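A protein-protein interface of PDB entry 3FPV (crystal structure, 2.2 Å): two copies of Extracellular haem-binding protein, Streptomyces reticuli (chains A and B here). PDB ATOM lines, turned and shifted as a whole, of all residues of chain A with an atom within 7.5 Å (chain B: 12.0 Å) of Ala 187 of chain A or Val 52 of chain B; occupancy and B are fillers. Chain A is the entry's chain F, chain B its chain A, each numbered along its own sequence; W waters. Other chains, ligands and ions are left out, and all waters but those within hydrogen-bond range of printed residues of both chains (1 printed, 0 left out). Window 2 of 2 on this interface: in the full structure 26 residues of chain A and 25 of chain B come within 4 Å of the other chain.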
ATOM      1  N   LYS A  72     -19.634  12.687 -20.760  1.00  0.00           N
ATOM      2  CA  LYS A  72     -19.339  13.472 -19.566  1.00  0.00           C
ATOM      3  C   LYS A  72     -20.485  14.420 -19.219  1.00  0.00           C
ATOM      4  O   LYS A  72     -20.918  14.493 -18.067  1.00  0.00           O
ATOM      5  CB  LYS A  72     -18.039  14.262 -19.753  1.00  0.00           C
ATOM      6  CG  LYS A  72     -17.732  15.234 -18.623  1.00  0.00           C
ATOM      7  CD  LYS A  72     -16.274  15.666 -18.642  1.00  0.00           C
ATOM      8  CE  LYS A  72     -16.100  16.996 -19.360  1.00  0.00           C
ATOM      9  NZ  LYS A  72     -14.917  16.986 -20.268  1.00  0.00           N
ATOM     10  N   ALA A  73     -20.973  15.141 -20.225  1.00  0.00           N
ATOM     11  CA  ALA A  73     -22.025  16.133 -20.027  1.00  0.00           C
ATOM     12  C   ALA A  73     -23.369  15.468 -19.747  1.00  0.00           C
ATOM     13  O   ALA A  73     -24.165  15.969 -18.953  1.00  0.00           O
ATOM     14  CB  ALA A  73     -22.125  17.049 -21.239  1.00  0.00           C
ATOM     15  N   ALA A  74     -23.610  14.336 -20.401  1.00  0.00           N
ATOM     16  CA  ALA A  74     -24.789  13.521 -20.128  1.00  0.00           C
ATOM     17  C   ALA A  74     -24.831  13.055 -18.672  1.00  0.00           C
ATOM     18  O   ALA A  74     -25.832  13.242 -17.980  1.00  0.00           O
ATOM     19  CB  ALA A  74     -24.840  12.328 -21.074  1.00  0.00           C
ATOM     20  N   ALA A  76     -23.223  14.041 -16.063  1.00  0.00           N
ATOM     21  CA  ALA A  76     -23.373  15.186 -15.170  1.00  0.00           C
ATOM     22  C   ALA A  76     -24.836  15.596 -14.999  1.00  0.00           C
ATOM     23  O   ALA A  76     -25.253  15.988 -13.909  1.00  0.00           O
ATOM     24  CB  ALA A  76     -22.549  16.360 -15.676  1.00  0.00           C
ATOM     25  N   ALA A  77     -25.604  15.506 -16.081  1.00  0.00           N
ATOM     26  CA  ALA A  77     -27.006  15.918 -16.064  1.00  0.00           C
ATOM     27  C   ALA A  77     -27.869  14.958 -15.245  1.00  0.00           C
ATOM     28  O   ALA A  77     -28.740  15.388 -14.489  1.00  0.00           O
ATOM     29  CB  ALA A  77     -27.541  16.039 -17.484  1.00  0.00           C
ATOM     30  N   ASN A 127     -30.406  26.471 -31.696  1.00  0.00           N
ATOM     31  CA  ASN A 127     -29.339  27.054 -30.883  1.00  0.00           C
ATOM     32  C   ASN A 127     -29.886  27.919 -29.745  1.00  0.00           C
ATOM     33  O   ASN A 127     -29.433  29.045 -29.526  1.00  0.00           O
ATOM     34  CB  ASN A 127     -28.373  27.853 -31.763  1.00  0.00           C
ATOM     35  CG  ASN A 127     -27.108  28.261 -31.029  1.00  0.00           C
ATOM     36  OD1 ASN A 127     -26.691  27.611 -30.068  1.00  0.00           O
ATOM     37  ND2 ASN A 127     -26.491  29.346 -31.481  1.00  0.00           N
ATOM     38  N   THR A 156     -31.055  22.114 -23.991  1.00  0.00           N
ATOM     39  CA  THR A 156     -30.116  23.235 -24.007  1.00  0.00           C
ATOM     40  C   THR A 156     -29.001  22.991 -25.027  1.00  0.00           C
ATOM     41  O   THR A 156     -28.539  21.859 -25.185  1.00  0.00           O
ATOM     42  CB  THR A 156     -29.522  23.500 -22.597  1.00  0.00           C
ATOM     43  OG1 THR A 156     -29.585  24.900 -22.300  1.00  0.00           O
ATOM     44  CG2 THR A 156     -28.076  23.030 -22.506  1.00  0.00           C
ATOM     45  N   PRO A 157     -28.581  24.052 -25.739  1.00  0.00           N
ATOM     46  CA  PRO A 157     -27.536  23.948 -26.753  1.00  0.00           C
ATOM     47  C   PRO A 157     -26.126  23.986 -26.167  1.00  0.00           C
ATOM     48  O   PRO A 157     -25.880  24.672 -25.173  1.00  0.00           O
ATOM     49  CB  PRO A 157     -27.776  25.182 -27.621  1.00  0.00           C
ATOM     50  CG  PRO A 157     -28.352  26.182 -26.690  1.00  0.00           C
ATOM     51  CD  PRO A 157     -29.108  25.424 -25.626  1.00  0.00           C
ATOM     52  N   VAL A 158     -25.212  23.248 -26.789  1.00  0.00           N
ATOM     53  CA  VAL A 158     -23.781  23.475 -26.626  1.00  0.00           C
ATOM     54  C   VAL A 158     -23.179  24.040 -27.907  1.00  0.00           C
ATOM     55  O   VAL A 158     -23.486  23.571 -29.003  1.00  0.00           O
ATOM     56  CB  VAL A 158     -23.048  22.169 -26.256  1.00  0.00           C
ATOM     57  CG1 VAL A 158     -21.553  22.414 -26.107  1.00  0.00           C
ATOM     58  CG2 VAL A 158     -23.627  21.581 -24.977  1.00  0.00           C
ATOM     59  N   THR A 159     -22.323  25.049 -27.767  1.00  0.00           N
ATOM     60  CA  THR A 159     -21.666  25.658 -28.922  1.00  0.00           C
ATOM     61  C   THR A 159     -20.174  25.347 -28.956  1.00  0.00           C
ATOM     62  O   THR A 159     -19.566  25.046 -27.929  1.00  0.00           O
ATOM     63  CB  THR A 159     -21.858  27.189 -28.954  1.00  0.00           C
ATOM     64  OG1 THR A 159     -21.302  27.769 -27.767  1.00  0.00           O
ATOM     65  CG2 THR A 159     -23.336  27.543 -29.049  1.00  0.00           C
ATOM     66  N   ALA A 160     -19.592  25.419 -30.149  1.00  0.00           N
ATOM     67  CA  ALA A 160     -18.149  25.555 -30.298  1.00  0.00           C
ATOM     68  C   ALA A 160     -17.815  26.644 -31.309  1.00  0.00           C
ATOM     69  O   ALA A 160     -18.281  26.603 -32.451  1.00  0.00           O
ATOM     70  CB  ALA A 160     -17.533  24.232 -30.724  1.00  0.00           C
ATOM     71  N   ALA A 163     -20.851  28.488 -33.063  1.00  0.00           N
ATOM     72  CA  ALA A 163     -21.800  27.620 -33.756  1.00  0.00           C
ATOM     73  C   ALA A 163     -22.278  26.488 -32.849  1.00  0.00           C
ATOM     74  O   ALA A 163     -21.494  25.935 -32.078  1.00  0.00           O
ATOM     75  CB  ALA A 163     -21.171  27.057 -35.019  1.00  0.00           C
ATOM     76  N   VAL A 165     -23.153  22.833 -31.736  1.00  0.00           N
ATOM     77  CA  VAL A 165     -22.547  21.553 -32.095  1.00  0.00           C
ATOM     78  C   VAL A 165     -23.288  20.359 -31.495  1.00  0.00           C
ATOM     79  O   VAL A 165     -23.236  19.255 -32.035  1.00  0.00           O
ATOM     80  CB  VAL A 165     -21.050  21.490 -31.708  1.00  0.00           C
ATOM     81  CG1 VAL A 165     -20.238  22.427 -32.587  1.00  0.00           C
ATOM     82  CG2 VAL A 165     -20.856  21.825 -30.234  1.00  0.00           C
ATOM     83  N   ALA A 166     -23.979  20.587 -30.381  1.00  0.00           N
ATOM     84  CA  ALA A 166     -24.794  19.545 -29.768  1.00  0.00           C
ATOM     85  C   ALA A 166     -25.967  20.132 -28.988  1.00  0.00           C
ATOM     86  O   ALA A 166     -25.976  21.318 -28.657  1.00  0.00           O
ATOM     87  CB  ALA A 166     -23.942  18.659 -28.873  1.00  0.00           C
ATOM     88  N   ILE A 168     -28.141  19.081 -25.368  1.00  0.00           N
ATOM     89  CA  ILE A 168     -28.430  18.209 -24.236  1.00  0.00           C
ATOM     90  C   ILE A 168     -29.893  18.318 -23.819  1.00  0.00           C
ATOM     91  O   ILE A 168     -30.389  19.408 -23.537  1.00  0.00           O
ATOM     92  CB  ILE A 168     -27.517  18.514 -23.032  1.00  0.00           C
ATOM     93  CG1 ILE A 168     -26.058  18.600 -23.486  1.00  0.00           C
ATOM     94  CG2 ILE A 168     -27.675  17.444 -21.957  1.00  0.00           C
ATOM     95  CD1 ILE A 168     -25.143  19.266 -22.486  1.00  0.00           C
ATOM     96  N   GLN A 181     -32.807  22.762 -15.815  1.00  0.00           N
ATOM     97  CA  GLN A 181     -31.819  23.032 -14.778  1.00  0.00           C
ATOM     98  C   GLN A 181     -30.723  21.971 -14.775  1.00  0.00           C
ATOM     99  O   GLN A 181     -29.536  22.291 -14.683  1.00  0.00           O
ATOM    100  CB  GLN A 181     -32.490  23.105 -13.403  1.00  0.00           C
ATOM    101  CG  GLN A 181     -31.637  23.757 -12.324  1.00  0.00           C
ATOM    102  CD  GLN A 181     -32.099  23.407 -10.922  1.00  0.00           C
ATOM    103  OE1 GLN A 181     -31.330  22.884 -10.114  1.00  0.00           O
ATOM    104  NE2 GLN A 181     -33.362  23.696 -10.624  1.00  0.00           N
ATOM    105  N   TYR A 182     -31.127  20.710 -14.882  1.00  0.00           N
ATOM    106  CA  TYR A 182     -30.179  19.602 -14.944  1.00  0.00           C
ATOM    107  C   TYR A 182     -29.472  19.552 -16.295  1.00  0.00           C
ATOM    108  O   TYR A 182     -28.323  19.119 -16.385  1.00  0.00           O
ATOM    109  CB  TYR A 182     -30.881  18.269 -14.671  1.00  0.00           C
ATOM    110  CG  TYR A 182     -31.873  18.303 -13.527  1.00  0.00           C
ATOM    111  CD1 TYR A 182     -31.605  19.016 -12.365  1.00  0.00           C
ATOM    112  CD2 TYR A 182     -33.078  17.615 -13.609  1.00  0.00           C
ATOM    113  CE1 TYR A 182     -32.511  19.048 -11.319  1.00  0.00           C
ATOM    114  CE2 TYR A 182     -33.990  17.639 -12.566  1.00  0.00           C
ATOM    115  CZ  TYR A 182     -33.700  18.358 -11.425  1.00  0.00           C
ATOM    116  OH  TYR A 182     -34.603  18.386 -10.387  1.00  0.00           O
ATOM    117  N   ALA A 183     -30.163  19.994 -17.342  1.00  0.00           N
ATOM    118  CA  ALA A 183     -29.557  20.108 -18.664  1.00  0.00           C
ATOM    119  C   ALA A 183     -28.431  21.139 -18.670  1.00  0.00           C
ATOM    120  O   ALA A 183     -27.367  20.902 -19.241  1.00  0.00           O
ATOM    121  CB  ALA A 183     -30.611  20.461 -19.704  1.00  0.00           C
ATOM    122  N   ARG A 184     -28.674  22.276 -18.026  1.00  0.00           N
ATOM    123  CA  ARG A 184     -27.664  23.324 -17.898  1.00  0.00           C
ATOM    124  C   ARG A 184     -26.450  22.837 -17.115  1.00  0.00           C
ATOM    125  O   ARG A 184     -25.310  23.168 -17.450  1.00  0.00           O
ATOM    126  CB  ARG A 184     -28.260  24.564 -17.225  1.00  0.00           C
ATOM    127  CG  ARG A 184     -29.136  25.408 -18.138  1.00  0.00           C
ATOM    128  CD  ARG A 184     -29.381  26.796 -17.558  1.00  0.00           C
ATOM    129  NE  ARG A 184     -29.849  26.751 -16.174  1.00  0.00           N
ATOM    130  CZ  ARG A 184     -31.122  26.611 -15.817  1.00  0.00           C
ATOM    131  NH1 ARG A 184     -32.067  26.498 -16.741  1.00  0.00           N
ATOM    132  NH2 ARG A 184     -31.452  26.581 -14.532  1.00  0.00           N
ATOM    133  N   ALA A 185     -26.705  22.051 -16.073  1.00  0.00           N
ATOM    134  CA  ALA A 185     -25.647  21.518 -15.221  1.00  0.00           C
ATOM    135  C   ALA A 185     -24.739  20.563 -15.990  1.00  0.00           C
ATOM    136  O   ALA A 185     -23.523  20.559 -15.798  1.00  0.00           O
ATOM    137  CB  ALA A 185     -26.246  20.822 -14.012  1.00  0.00           C
ATOM    138  N   GLY A 186     -25.339  19.757 -16.861  1.00  0.00           N
ATOM    139  CA  GLY A 186     -24.581  18.907 -17.772  1.00  0.00           C
ATOM    140  C   GLY A 186     -23.704  19.698 -18.723  1.00  0.00           C
ATOM    141  O   GLY A 186     -22.543  19.353 -18.941  1.00  0.00           O
ATOM    142  N   ALA A 187     -24.260  20.765 -19.288  1.00  0.00           N
ATOM    143  CA  ALA A 187     -23.523  21.628 -20.205  1.00  0.00           C
ATOM    144  C   ALA A 187     -22.347  22.315 -19.517  1.00  0.00           C
ATOM    145  O   ALA A 187     -21.354  22.660 -20.161  1.00  0.00           O
ATOM    146  CB  ALA A 187     -24.456  22.659 -20.824  1.00  0.00           C
ATOM    147  N   ALA A 188     -22.464  22.507 -18.207  1.00  0.00           N
ATOM    148  CA  ALA A 188     -21.563  23.388 -17.472  1.00  0.00           C
ATOM    149  C   ALA A 188     -20.220  22.718 -17.206  1.00  0.00           C
ATOM    150  O   ALA A 188     -19.239  23.389 -16.884  1.00  0.00           O
ATOM    151  CB  ALA A 188     -22.205  23.833 -16.167  1.00  0.00           C
ATOM    152  N   VAL A 189     -20.178  21.397 -17.348  1.00  0.00           N
ATOM    153  CA  VAL A 189     -18.937  20.650 -17.168  1.00  0.00           C
ATOM    154  C   VAL A 189     -18.072  20.669 -18.427  1.00  0.00           C
ATOM    155  O   VAL A 189     -16.947  20.168 -18.424  1.00  0.00           O
ATOM    156  CB  VAL A 189     -19.206  19.189 -16.749  1.00  0.00           C
ATOM    157  CG1 VAL A 189     -20.194  19.143 -15.594  1.00  0.00           C
ATOM    158  CG2 VAL A 189     -19.717  18.377 -17.929  1.00  0.00           C
ATOM    159  N   LEU A 190     -18.606  21.246 -19.500  1.00  0.00           N
ATOM    160  CA  LEU A 190     -17.791  21.691 -20.627  1.00  0.00           C
ATOM    161  C   LEU A 190     -17.477  23.185 -20.517  1.00  0.00           C
ATOM    162  O   LEU A 190     -18.127  23.904 -19.758  1.00  0.00           O
ATOM    163  CB  LEU A 190     -18.501  21.393 -21.949  1.00  0.00           C
ATOM    164  CG  LEU A 190     -19.256  20.063 -22.032  1.00  0.00           C
ATOM    165  CD1 LEU A 190     -20.335  20.125 -23.101  1.00  0.00           C
ATOM    166  CD2 LEU A 190     -18.300  18.910 -22.296  1.00  0.00           C
ATOM    167  N   GLY A 191     -16.486  23.652 -21.274  1.00  0.00           N
ATOM    168  CA  GLY A 191     -15.253  22.904 -21.520  1.00  0.00           C
ATOM    169  C   GLY A 191     -14.457  22.569 -20.271  1.00  0.00           C
ATOM    170  O   GLY A 191     -14.910  21.800 -19.423  1.00  0.00           O
ATOM    171  N   HIS A 192     -13.255  23.128 -20.157  1.00  0.00           N
ATOM    172  CA  HIS A 192     -13.047  24.573 -20.040  1.00  0.00           C
ATOM    173  C   HIS A 192     -11.697  24.859 -19.394  1.00  0.00           C
ATOM    174  O   HIS A 192     -10.657  24.434 -19.898  1.00  0.00           O
ATOM    175  CB  HIS A 192     -14.168  25.255 -19.242  1.00  0.00           C
ATOM    176  CG  HIS A 192     -14.649  24.466 -18.064  1.00  0.00           C
ATOM    177  ND1 HIS A 192     -13.859  23.546 -17.406  1.00  0.00           N
ATOM    178  CD2 HIS A 192     -15.845  24.455 -17.428  1.00  0.00           C
ATOM    179  CE1 HIS A 192     -14.549  23.002 -16.420  1.00  0.00           C
ATOM    180  NE2 HIS A 192     -15.756  23.539 -16.409  1.00  0.00           N
ATOM    181  OXT HIS A 192     -11.612  25.516 -18.356  1.00  0.00           O
ATOM    182  N   VAL B  52     -22.990  28.508 -23.654  1.00  0.00           N
ATOM    183  CA  VAL B  52     -22.150  27.396 -23.119  1.00  0.00           C
ATOM    184  C   VAL B  52     -21.245  26.812 -24.200  1.00  0.00           C
ATOM    185  O   VAL B  52     -21.717  26.174 -25.141  1.00  0.00           O
ATOM    186  CB  VAL B  52     -23.013  26.269 -22.524  1.00  0.00           C
ATOM    187  CG1 VAL B  52     -22.699  26.088 -21.048  1.00  0.00           C
ATOM    188  CG2 VAL B  52     -24.493  26.562 -22.734  1.00  0.00           C
ATOM    189  N   ALA B  53     -19.940  27.036 -24.053  1.00  0.00           N
ATOM    190  CA  ALA B  53     -18.980  26.725 -25.107  1.00  0.00           C
ATOM    191  C   ALA B  53     -18.127  25.516 -24.733  1.00  0.00           C
ATOM    192  O   ALA B  53     -17.600  25.436 -23.622  1.00  0.00           O
ATOM    193  CB  ALA B  53     -18.099  27.931 -25.397  1.00  0.00           C
ATOM    194  N   ALA B  54     -17.996  24.580 -25.668  1.00  0.00           N
ATOM    195  CA  ALA B  54     -16.955  23.558 -25.602  1.00  0.00           C
ATOM    196  C   ALA B  54     -15.657  24.003 -26.271  1.00  0.00           C
ATOM    197  O   ALA B  54     -15.673  24.765 -27.240  1.00  0.00           O
ATOM    198  CB  ALA B  54     -17.453  22.258 -26.220  1.00  0.00           C
ATOM    199  N   ARG B  55     -14.536  23.515 -25.747  1.00  0.00           N
ATOM    200  CA  ARG B  55     -13.255  23.587 -26.445  1.00  0.00           C
ATOM    201  C   ARG B  55     -12.273  22.547 -25.908  1.00  0.00           C
ATOM    202  O   ARG B  55     -12.622  21.735 -25.051  1.00  0.00           O
ATOM    203  CB  ARG B  55     -12.654  24.987 -26.317  1.00  0.00           C
ATOM    204  CG  ARG B  55     -12.858  25.623 -24.952  1.00  0.00           C
ATOM    205  CD  ARG B  55     -11.759  26.620 -24.649  1.00  0.00           C
ATOM    206  NE  ARG B  55     -10.637  26.001 -23.951  1.00  0.00           N
ATOM    207  CZ  ARG B  55     -10.466  26.036 -22.632  1.00  0.00           C
ATOM    208  NH1 ARG B  55      -9.414  25.448 -22.081  1.00  0.00           N
ATOM    209  NH2 ARG B  55     -11.347  26.664 -21.865  1.00  0.00           N
ATOM    210  N   GLY B  56     -11.045  22.576 -26.416  1.00  0.00           N
ATOM    211  CA  GLY B  56     -10.742  22.014 -27.727  1.00  0.00           C
ATOM    212  C   GLY B  56     -10.540  20.512 -27.678  1.00  0.00           C
ATOM    213  O   GLY B  56     -10.713  19.819 -28.681  1.00  0.00           O
ATOM    214  N   GLU B  58     -12.367  18.445 -26.086  1.00  0.00           N
ATOM    215  CA  GLU B  58     -13.678  17.810 -26.152  1.00  0.00           C
ATOM    216  C   GLU B  58     -14.330  18.024 -27.513  1.00  0.00           C
ATOM    217  O   GLU B  58     -15.445  17.562 -27.756  1.00  0.00           O
ATOM    218  CB  GLU B  58     -14.589  18.358 -25.054  1.00  0.00           C
ATOM    219  CG  GLU B  58     -13.866  18.773 -23.787  1.00  0.00           C
ATOM    220  CD  GLU B  58     -14.672  19.750 -22.960  1.00  0.00           C
ATOM    221  OE1 GLU B  58     -15.183  20.734 -23.534  1.00  0.00           O
ATOM    222  OE2 GLU B  58     -14.798  19.531 -21.736  1.00  0.00           O
ATOM    223  N   LEU B  59     -13.627  18.728 -28.395  1.00  0.00           N
ATOM    224  CA  LEU B  59     -14.021  18.833 -29.795  1.00  0.00           C
ATOM    225  C   LEU B  59     -13.350  17.779 -30.667  1.00  0.00           C
ATOM    226  O   LEU B  59     -12.201  17.402 -30.432  1.00  0.00           O
ATOM    227  CB  LEU B  59     -13.705  20.228 -30.334  1.00  0.00           C
ATOM    228  CG  LEU B  59     -14.291  21.411 -29.562  1.00  0.00           C
ATOM    229  CD1 LEU B  59     -13.925  22.722 -30.240  1.00  0.00           C
ATOM    230  CD2 LEU B  59     -15.798  21.270 -29.428  1.00  0.00           C
HETATM  231  O   HOH W   1     -11.865  21.685 -22.104  1.00  0.00           O
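The backbone carbonyl oxygen (O) of Gly 191 of chain A sits close to the side-chain carboxylate (OE2) of Glu 58 of chain B (3.2 Å).
The backbone NH (N) of Ala 54 of chain B sits at hydrogen-bond distance from the backbone carbonyl oxygen (O) of Thr 159 of chain A.
The backbone carbonyl oxygen (O) of Val 52 of chain B is in hydrogen-bond range of the backbone NH (N) of Thr 159 of chain A.
The side-chain carboxylate (OE2) of Glu 58 of chain B lies within salt-bridge range of the side-chain amino group (NZ) of Lys 72 of chain A (2.9 Å).
NH1 of Arg 55 of chain B is in salt-bridge range of O of His 192 of chain A (2.7 Å).
The backbone carbonyl oxygen (O) of Ala 53 of chain B sits at hydrogen-bond distance from the backbone NH (N) of Gly 191 of chain A (3.2 Å).
No position is printed for both chains.
Of the 15 pairs that touch across the chains among the printed residues, none has its exchanged pair printed and touching as well.
Val 52 of chain B touches Pro 157 of chain A (CG2 to O, 3.4 Å).
Val 52 of chain B touches Val 158 of chain A (O to CA, 3.7 Å).
Thr 159 of chain A touches Ala 53 of chain B (O to CA, 3.3 Å).
CB of Ala 160 of chain A touches O of Ala 54 of chain B (3.99 Å).
Leu 59 of chain B touches Ala 160 of chain A.
Val 52 of chain B touches Ala 187 of chain A (CG1 to O, 3.8 Å).
Glu 58 of chain B touches Val 189 of chain A (OE2 to O, 3.999 Å).
Leu 190 of chain A touches Ala 53 of chain B (C to O, 3.8 Å).
Leu 190 of chain A touches Glu 58 of chain B (CD2 to OE2, 3.6 Å).
N of Val 165 of chain A is in hydrogen-bond range of O of Val 158 of chain A (2.9 Å).
N of Val 158 of chain A lies within hydrogen-bond range of O of Ala 166 of chain A.
Hydrophobic or aromatic side chains of chain B within 4 Å of the printed part of chain A: Val 52, Ala 53, Ala 54 and Leu 59.
Of the 27 printed residues of chain A, 10 touch a printed residue of chain B.
Printed residues of chain A that touch a printed residue of chain B: Lys 72, Pro 157, Val 158, Thr 159, Ala 160, Ala 187, Val 189, Leu 190, Gly 191 and His 192.
Hydrophobic or aromatic side chains of chain A within 4 Å of the printed part of chain B: Val 158, Ala 160, Ala 187 and Leu 190.
Along chain A the printed residues that touch a printed residue of chain B span positions 72 to 192.
Among the printed residues, 15 pairs touch across the chains.
No residue of chain B comes within 4 Å of Ala 76 of chain A.
No residue of chain B comes within 4 Å of Thr 156 of chain A.
Printed residues of chain B within 4 Å of Pro 157 of chain A: Val 52.
Of chain B, only Val 52 (3.7 Å) comes within 4 Å of Val 158 of chain A.
Of chain B, only Val 52, Ala 53 and Ala 54 come within 4 Å of Thr 159 of chain A.
Ala 166 of chain A touches none of the printed residues of chain B.
No residue of chain B comes within 4 Å of Ile 168 of chain A.
No residue of chain B comes within 4 Å of Ala 183 of chain A.
No residue of chain B comes within 4 Å of Gly 186 of chain A.
Ala 187 of chain A touches just one residue of chain B: Val 52 (3.8 Å).
No residue of chain B comes within 4 Å of Ala 188 of chain A.
Of the printed residues of chain B, Val 189 of chain A touches Glu 58.
Leu 190 of chain A touches two residues of chain B.
Printed residues of chain B within 4 Å of Gly 191 of chain A: Ala 53 and Glu 58.
Of chain A, only Pro 157, Val 158, Thr 159 and Ala 187 come within 4 Å of Val 52 of chain B.
Printed residues of chain A within 4 Å of Ala 53 of chain B: Thr 159 (3.3 Å), Leu 190 (3.8 Å) and Gly 191 (3.2 Å).
Printed residues of chain A within 4 Å of Ala 54 of chain B: Thr 159 and Ala 160.
Of the printed residues of chain A, Arg 55 of chain B touches His 192 (2.7 Å).
Of the printed residues of chain A, Leu 59 of chain B touches Ala 160 (3.7 Å).
The nearest residue of chain A that does not touch Val 52 of chain B is Ala 188 of chain A (4.6 Å).
The nearest printed residue of chain A that does not touch Ala 53 of chain B is Val 158 of chain A (4.8 Å).
Water W1 lies within hydrogen-bond range of N of His 192 of chain A (2.8 Å) and O of Arg 55 of chain B (3.0 Å).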
